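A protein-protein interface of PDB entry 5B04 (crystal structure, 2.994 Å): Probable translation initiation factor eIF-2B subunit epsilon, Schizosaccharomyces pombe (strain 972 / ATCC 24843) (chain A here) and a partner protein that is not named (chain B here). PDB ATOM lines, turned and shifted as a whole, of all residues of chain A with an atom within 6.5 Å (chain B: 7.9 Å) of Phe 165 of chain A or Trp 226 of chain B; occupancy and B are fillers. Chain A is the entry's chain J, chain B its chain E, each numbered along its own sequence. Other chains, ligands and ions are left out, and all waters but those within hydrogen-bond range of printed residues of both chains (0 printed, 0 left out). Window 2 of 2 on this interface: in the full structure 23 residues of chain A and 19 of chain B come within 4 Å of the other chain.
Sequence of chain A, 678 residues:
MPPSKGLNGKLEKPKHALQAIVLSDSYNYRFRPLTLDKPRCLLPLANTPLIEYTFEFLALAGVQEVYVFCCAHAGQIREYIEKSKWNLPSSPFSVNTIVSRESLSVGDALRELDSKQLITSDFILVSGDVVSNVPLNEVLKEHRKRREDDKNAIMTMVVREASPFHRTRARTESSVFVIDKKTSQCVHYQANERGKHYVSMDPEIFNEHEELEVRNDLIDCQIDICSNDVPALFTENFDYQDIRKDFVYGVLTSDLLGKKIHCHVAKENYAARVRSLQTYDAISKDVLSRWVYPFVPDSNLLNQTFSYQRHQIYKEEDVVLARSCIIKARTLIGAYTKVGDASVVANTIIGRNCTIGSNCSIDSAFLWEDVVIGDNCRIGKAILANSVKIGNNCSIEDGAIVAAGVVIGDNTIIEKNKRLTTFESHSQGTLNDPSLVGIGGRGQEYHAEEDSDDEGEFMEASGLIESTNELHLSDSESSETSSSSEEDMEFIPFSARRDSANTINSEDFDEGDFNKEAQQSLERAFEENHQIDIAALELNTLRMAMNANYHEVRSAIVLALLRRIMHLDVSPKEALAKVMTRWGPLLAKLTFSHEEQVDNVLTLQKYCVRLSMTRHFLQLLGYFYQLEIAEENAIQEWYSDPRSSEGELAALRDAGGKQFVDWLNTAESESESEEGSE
Hydrophobic or aromatic side chains of chain B that line the printed part of chain A: Met 222, Trp 226 and Pro 229. Of the 10 printed residues of chain A, 5 touch a printed residue of chain B. Hydrophobic or aromatic side chains of chain A that line the printed part of chain B: Pro 164 and Phe 165. Among the printed residues, 8 pairs touch across the chains.
OG of Ser 174 of chain A lies within hydrogen-bond range of NH2 of Arg 169 of chain A (3.2 Å). ND2 of Asn 192 of chain A lies within hydrogen-bond range of OD1 of Asn 216 of chain A. The side-chain hydroxyl of Ser 174 of chain A lies within hydrogen-bond range of the side-chain amide nitrogen of Asn 192 of chain A, 2.9 Å away. OD1 of Asn 216 of chain A lies within hydrogen-bond range of NH2 of Arg 169 of chain A. The side-chain amide nitrogen (ND2) of Asn 192 of chain A lies close to the guanidinium group (NH2) of Arg 169 of chain A (3.2 Å). NE of Arg 169 of chain A is in hydrogen-bond range of O of Pro 164 of chain A (2.9 Å).
Among the printed residues, pairs that only touch across the chains: Pro 164 of chain A with Trp 226 of chain B, Pro 164 of chain A with Pro 229 of chain B, Phe 165 of chain A with Trp 226 of chain B, Ser 174 of chain A with Trp 226 of chain B and Asn 216 of chain A with Trp 226 of chain B.
The side-chain sulfur of Met 222 of chain B lies close to the side-chain amide oxygen of Asn 192 of chain A. The side-chain amide nitrogen of Asn 216 of chain A lies within hydrogen-bond range of the backbone carbonyl oxygen of Leu 225 of chain B (2.8 Å). The backbone NH (N) of Asn 216 of chain A sits at hydrogen-bond distance from the backbone carbonyl oxygen (O) of Pro 229 of chain B, 2.8 Å away.
Of the printed residues of chain B, Pro 164 of chain A touches Trp 226 (3.6 Å) and Pro 229 (3.9 Å). Of the printed residues of chain B, Ser 174 of chain A touches Trp 226 (3.6 Å). Of the printed residues of chain A, Met 222 of chain B touches Asn 192 (3.5 Å). Of the printed residues of chain A, Trp 226 of chain B touches Pro 164, Phe 165, Ser 174 and Asn 216. His 228 of chain B touches none of the printed residues of chain A. The nearest residue of chain B that does not touch Phe 165 of chain A is Lys 227 of chain B (5.0 Å). The nearest printed residue of chain A that does not touch Trp 226 of chain B is Asn 192 of chain A (4.01 Å).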
ATOM      1  N   SER A 163      -4.562  12.446   4.362  1.00  0.00           N
ATOM      2  CA  SER A 163      -3.361  12.902   4.992  1.00  0.00           C
ATOM      3  C   SER A 163      -2.475  11.701   5.029  1.00  0.00           C
ATOM      4  O   SER A 163      -2.971  10.595   4.974  1.00  0.00           O
ATOM      5  CB  SER A 163      -3.653  13.335   6.405  1.00  0.00           C
ATOM      6  OG  SER A 163      -4.042  12.224   7.169  1.00  0.00           O
ATOM      7  N   PRO A 164      -1.100  11.953   5.113  1.00  0.00           N
ATOM      8  CA  PRO A 164      -0.285  10.738   5.037  1.00  0.00           C
ATOM      9  C   PRO A 164      -0.532   9.728   6.132  1.00  0.00           C
ATOM     10  O   PRO A 164      -0.506   8.556   5.836  1.00  0.00           O
ATOM     11  CB  PRO A 164       1.145  11.249   5.111  1.00  0.00           C
ATOM     12  CG  PRO A 164       1.063  12.516   5.825  1.00  0.00           C
ATOM     13  CD  PRO A 164      -0.101  13.126   5.170  1.00  0.00           C
ATOM     14  N   PHE A 165      -0.736  10.142   7.367  1.00  0.00           N
ATOM     15  CA  PHE A 165      -0.812   9.194   8.454  1.00  0.00           C
ATOM     16  C   PHE A 165      -2.231   8.815   8.705  1.00  0.00           C
ATOM     17  O   PHE A 165      -2.579   8.222   9.698  1.00  0.00           O
ATOM     18  CB  PHE A 165      -0.203   9.794   9.693  1.00  0.00           C
ATOM     19  CG  PHE A 165       1.248  10.055   9.553  1.00  0.00           C
ATOM     20  CD1 PHE A 165       2.130   9.011   9.465  1.00  0.00           C
ATOM     21  CD2 PHE A 165       1.719  11.333   9.475  1.00  0.00           C
ATOM     22  CE1 PHE A 165       3.471   9.235   9.323  1.00  0.00           C
ATOM     23  CE2 PHE A 165       3.058  11.573   9.329  1.00  0.00           C
ATOM     24  CZ  PHE A 165       3.936  10.520   9.254  1.00  0.00           C
ATOM     25  N   HIS A 166      -3.058   9.208   7.781  1.00  0.00           N
ATOM     26  CA  HIS A 166      -4.502   9.041   7.916  1.00  0.00           C
ATOM     27  C   HIS A 166      -4.843   7.609   8.316  1.00  0.00           C
ATOM     28  O   HIS A 166      -4.225   6.657   7.838  1.00  0.00           O
ATOM     29  CB  HIS A 166      -5.210   9.412   6.611  1.00  0.00           C
ATOM     30  CG  HIS A 166      -6.686   9.614   6.761  1.00  0.00           C
ATOM     31  ND1 HIS A 166      -7.556   8.579   7.022  1.00  0.00           N
ATOM     32  CD2 HIS A 166      -7.444  10.734   6.684  1.00  0.00           C
ATOM     33  CE1 HIS A 166      -8.787   9.052   7.103  1.00  0.00           C
ATOM     34  NE2 HIS A 166      -8.747  10.356   6.901  1.00  0.00           N
ATOM     35  N   ARG A 167      -5.828   7.468   9.196  1.00  0.00           N
ATOM     36  CA  ARG A 167      -6.193   6.170   9.755  1.00  0.00           C
ATOM     37  C   ARG A 167      -6.678   5.184   8.693  1.00  0.00           C
ATOM     38  O   ARG A 167      -6.373   3.994   8.758  1.00  0.00           O
ATOM     39  CB  ARG A 167      -7.268   6.348  10.830  1.00  0.00           C
ATOM     40  CG  ARG A 167      -7.696   5.057  11.503  1.00  0.00           C
ATOM     41  CD  ARG A 167      -8.702   5.323  12.609  1.00  0.00           C
ATOM     42  NE  ARG A 167      -9.105   4.094  13.286  1.00  0.00           N
ATOM     43  CZ  ARG A 167      -9.832   4.058  14.397  1.00  0.00           C
ATOM     44  NH1 ARG A 167     -10.238   5.187  14.962  1.00  0.00           N
ATOM     45  NH2 ARG A 167     -10.152   2.894  14.945  1.00  0.00           N
ATOM     46  N   THR A 168      -7.427   5.684   7.716  1.00  0.00           N
ATOM     47  CA  THR A 168      -7.974   4.837   6.661  1.00  0.00           C
ATOM     48  C   THR A 168      -6.927   4.572   5.578  1.00  0.00           C
ATOM     49  O   THR A 168      -7.158   3.803   4.645  1.00  0.00           O
ATOM     50  CB  THR A 168      -9.229   5.470   6.027  1.00  0.00           C
ATOM     51  OG1 THR A 168      -9.965   6.183   7.028  1.00  0.00           O
ATOM     52  CG2 THR A 168     -10.123   4.401   5.415  1.00  0.00           C
ATOM     53  N   ARG A 169      -5.770   5.213   5.713  1.00  0.00           N
ATOM     54  CA  ARG A 169      -4.666   5.012   4.782  1.00  0.00           C
ATOM     55  C   ARG A 169      -3.691   3.970   5.326  1.00  0.00           C
ATOM     56  O   ARG A 169      -2.796   4.290   6.109  1.00  0.00           O
ATOM     57  CB  ARG A 169      -3.947   6.337   4.516  1.00  0.00           C
ATOM     58  CG  ARG A 169      -2.741   6.239   3.592  1.00  0.00           C
ATOM     59  CD  ARG A 169      -2.157   7.618   3.327  1.00  0.00           C
ATOM     60  NE  ARG A 169      -0.713   7.580   3.111  1.00  0.00           N
ATOM     61  CZ  ARG A 169      -0.126   7.744   1.931  1.00  0.00           C
ATOM     62  NH1 ARG A 169      -0.858   7.963   0.848  1.00  0.00           N
ATOM     63  NH2 ARG A 169       1.195   7.695   1.833  1.00  0.00           N
ATOM     64  N   SER A 174      -1.057   3.260   1.213  1.00  0.00           N
ATOM     65  CA  SER A 174       0.090   4.151   1.345  1.00  0.00           C
ATOM     66  C   SER A 174       1.014   4.027   0.141  1.00  0.00           C
ATOM     67  O   SER A 174       1.817   3.098   0.054  1.00  0.00           O
ATOM     68  CB  SER A 174       0.861   3.855   2.633  1.00  0.00           C
ATOM     69  OG  SER A 174       1.933   4.764   2.806  1.00  0.00           O
ATOM     70  N   ASN A 192       4.538   2.279  -0.695  1.00  0.00           N
ATOM     71  CA  ASN A 192       5.395   2.687   0.405  1.00  0.00           C
ATOM     72  C   ASN A 192       5.869   1.522   1.243  1.00  0.00           C
ATOM     73  O   ASN A 192       5.178   1.075   2.162  1.00  0.00           O
ATOM     74  CB  ASN A 192       4.683   3.706   1.288  1.00  0.00           C
ATOM     75  CG  ASN A 192       4.762   5.102   0.721  1.00  0.00           C
ATOM     76  OD1 ASN A 192       5.797   5.500   0.186  1.00  0.00           O
ATOM     77  ND2 ASN A 192       3.676   5.854   0.830  1.00  0.00           N
ATOM     78  N   ASN A 216       2.051  12.167  -1.322  1.00  0.00           N
ATOM     79  CA  ASN A 216       2.133  11.117  -0.315  1.00  0.00           C
ATOM     80  C   ASN A 216       0.909  11.190   0.596  1.00  0.00           C
ATOM     81  O   ASN A 216       0.878  10.607   1.680  1.00  0.00           O
ATOM     82  CB  ASN A 216       3.430  11.256   0.490  1.00  0.00           C
ATOM     83  CG  ASN A 216       3.672  10.087   1.427  1.00  0.00           C
ATOM     84  OD1 ASN A 216       3.209   8.973   1.183  1.00  0.00           O
ATOM     85  ND2 ASN A 216       4.396  10.340   2.510  1.00  0.00           N
ATOM     86  N   ARG B 221      14.052  12.206  -0.833  1.00  0.00           N
ATOM     87  CA  ARG B 221      14.085  11.331   0.331  1.00  0.00           C
ATOM     88  C   ARG B 221      12.669  11.136   0.859  1.00  0.00           C
ATOM     89  O   ARG B 221      11.929  12.105   1.042  1.00  0.00           O
ATOM     90  CB  ARG B 221      14.998  11.897   1.420  1.00  0.00           C
ATOM     91  CG  ARG B 221      16.148  10.972   1.800  1.00  0.00           C
ATOM     92  CD  ARG B 221      17.055  11.601   2.848  1.00  0.00           C
ATOM     93  NE  ARG B 221      18.160  12.341   2.244  1.00  0.00           N
ATOM     94  CZ  ARG B 221      19.354  11.821   1.979  1.00  0.00           C
ATOM     95  NH1 ARG B 221      19.605  10.550   2.267  1.00  0.00           N
ATOM     96  NH2 ARG B 221      20.299  12.568   1.427  1.00  0.00           N
ATOM     97  N   MET B 222      12.292   9.882   1.094  1.00  0.00           N
ATOM     98  CA  MET B 222      10.954   9.553   1.576  1.00  0.00           C
ATOM     99  C   MET B 222      10.689  10.201   2.929  1.00  0.00           C
ATOM    100  O   MET B 222       9.543  10.480   3.284  1.00  0.00           O
ATOM    101  CB  MET B 222      10.774   8.037   1.673  1.00  0.00           C
ATOM    102  CG  MET B 222       9.356   7.599   2.003  1.00  0.00           C
ATOM    103  SD  MET B 222       8.190   8.023   0.697  1.00  0.00           S
ATOM    104  CE  MET B 222       8.809   7.002  -0.635  1.00  0.00           C
ATOM    105  N   SER B 223      11.762  10.437   3.677  1.00  0.00           N
ATOM    106  CA  SER B 223      11.681  11.105   4.969  1.00  0.00           C
ATOM    107  C   SER B 223      11.012  12.467   4.846  1.00  0.00           C
ATOM    108  O   SER B 223      10.138  12.817   5.641  1.00  0.00           O
ATOM    109  CB  SER B 223      13.078  11.266   5.573  1.00  0.00           C
ATOM    110  OG  SER B 223      13.847  12.197   4.829  1.00  0.00           O
ATOM    111  N   LEU B 224      11.421  13.227   3.836  1.00  0.00           N
ATOM    112  CA  LEU B 224      10.933  14.588   3.661  1.00  0.00           C
ATOM    113  C   LEU B 224       9.471  14.612   3.226  1.00  0.00           C
ATOM    114  O   LEU B 224       8.778  15.591   3.478  1.00  0.00           O
ATOM    115  CB  LEU B 224      11.807  15.344   2.650  1.00  0.00           C
ATOM    116  CG  LEU B 224      11.327  16.692   2.094  1.00  0.00           C
ATOM    117  CD1 LEU B 224      12.487  17.670   2.000  1.00  0.00           C
ATOM    118  CD2 LEU B 224      10.666  16.540   0.731  1.00  0.00           C
ATOM    119  N   LEU B 225       9.001  13.541   2.589  1.00  0.00           N
ATOM    120  CA  LEU B 225       7.639  13.514   2.050  1.00  0.00           C
ATOM    121  C   LEU B 225       6.585  12.991   3.028  1.00  0.00           C
ATOM    122  O   LEU B 225       5.397  12.964   2.701  1.00  0.00           O
ATOM    123  CB  LEU B 225       7.583  12.685   0.767  1.00  0.00           C
ATOM    124  CG  LEU B 225       7.353  13.471  -0.529  1.00  0.00           C
ATOM    125  CD1 LEU B 225       8.585  14.264  -0.938  1.00  0.00           C
ATOM    126  CD2 LEU B 225       6.904  12.542  -1.645  1.00  0.00           C
ATOM    127  N   TRP B 226       7.006  12.587   4.222  1.00  0.00           N
ATOM    128  CA  TRP B 226       6.054  12.301   5.291  1.00  0.00           C
ATOM    129  C   TRP B 226       5.616  13.625   5.892  1.00  0.00           C
ATOM    130  O   TRP B 226       4.436  13.847   6.164  1.00  0.00           O
ATOM    131  CB  TRP B 226       6.665  11.383   6.345  1.00  0.00           C
ATOM    132  CG  TRP B 226       6.804   9.984   5.852  1.00  0.00           C
ATOM    133  CD1 TRP B 226       7.963   9.302   5.631  1.00  0.00           C
ATOM    134  CD2 TRP B 226       5.739   9.101   5.487  1.00  0.00           C
ATOM    135  NE1 TRP B 226       7.685   8.040   5.162  1.00  0.00           N
ATOM    136  CE2 TRP B 226       6.327   7.893   5.064  1.00  0.00           C
ATOM    137  CE3 TRP B 226       4.345   9.211   5.485  1.00  0.00           C
ATOM    138  CZ2 TRP B 226       5.569   6.803   4.642  1.00  0.00           C
ATOM    139  CZ3 TRP B 226       3.595   8.130   5.065  1.00  0.00           C
ATOM    140  CH2 TRP B 226       4.208   6.942   4.649  1.00  0.00           C
ATOM    141  N   LYS B 227       6.590  14.505   6.086  1.00  0.00           N
ATOM    142  CA  LYS B 227       6.322  15.922   6.259  1.00  0.00           C
ATOM    143  C   LYS B 227       5.983  16.378   4.848  1.00  0.00           C
ATOM    144  O   LYS B 227       6.294  15.666   3.910  1.00  0.00           O
ATOM    145  CB  LYS B 227       7.535  16.683   6.824  1.00  0.00           C
ATOM    146  CG  LYS B 227       7.933  16.413   8.294  1.00  0.00           C
ATOM    147  CD  LYS B 227       7.603  15.013   8.803  1.00  0.00           C
ATOM    148  CE  LYS B 227       8.170  14.757  10.185  1.00  0.00           C
ATOM    149  NZ  LYS B 227       7.638  13.490  10.761  1.00  0.00           N
ATOM    150  N   HIS B 228       5.341  17.528   4.680  1.00  0.00           N
ATOM    151  CA  HIS B 228       5.099  18.066   3.336  1.00  0.00           C
ATOM    152  C   HIS B 228       4.640  17.024   2.306  1.00  0.00           C
ATOM    153  O   HIS B 228       5.358  16.762   1.340  1.00  0.00           O
ATOM    154  CB  HIS B 228       6.374  18.729   2.807  1.00  0.00           C
ATOM    155  CG  HIS B 228       6.978  19.726   3.747  1.00  0.00           C
ATOM    156  ND1 HIS B 228       6.350  20.904   4.086  1.00  0.00           N
ATOM    157  CD2 HIS B 228       8.156  19.721   4.413  1.00  0.00           C
ATOM    158  CE1 HIS B 228       7.115  21.582   4.923  1.00  0.00           C
ATOM    159  NE2 HIS B 228       8.216  20.886   5.138  1.00  0.00           N
ATOM    160  N   PRO B 229       3.459  16.419   2.508  1.00  0.00           N
ATOM    161  CA  PRO B 229       3.032  15.310   1.641  1.00  0.00           C
ATOM    162  C   PRO B 229       2.845  15.704   0.179  1.00  0.00           C
ATOM    163  O   PRO B 229       2.795  14.831  -0.687  1.00  0.00           O
ATOM    164  CB  PRO B 229       1.695  14.883   2.249  1.00  0.00           C
ATOM    165  CG  PRO B 229       1.206  16.084   2.978  1.00  0.00           C
ATOM    166  CD  PRO B 229       2.431  16.765   3.505  1.00  0.00           C
ATOM    167  N   ARG B 230       2.741  17.002  -0.087  1.00  0.00           N
ATOM    168  CA  ARG B 230       2.507  17.488  -1.441  1.00  0.00           C
ATOM    169  C   ARG B 230       3.602  18.446  -1.896  1.00  0.00           C
ATOM    170  O   ARG B 230       3.838  19.477  -1.266  1.00  0.00           O
ATOM    171  CB  ARG B 230       1.145  18.172  -1.525  1.00  0.00           C
ATOM    172  CG  ARG B 230      -0.005  17.322  -1.010  1.00  0.00           C
ATOM    173  CD  ARG B 230      -1.330  18.032  -1.196  1.00  0.00           C
ATOM    174  NE  ARG B 230      -1.505  18.484  -2.572  1.00  0.00           N
ATOM    175  CZ  ARG B 230      -2.584  19.116  -3.019  1.00  0.00           C
ATOM    176  NH1 ARG B 230      -3.593  19.373  -2.201  1.00  0.00           N
ATOM    177  NH2 ARG B 230      -2.652  19.490  -4.290  1.00  0.00           N
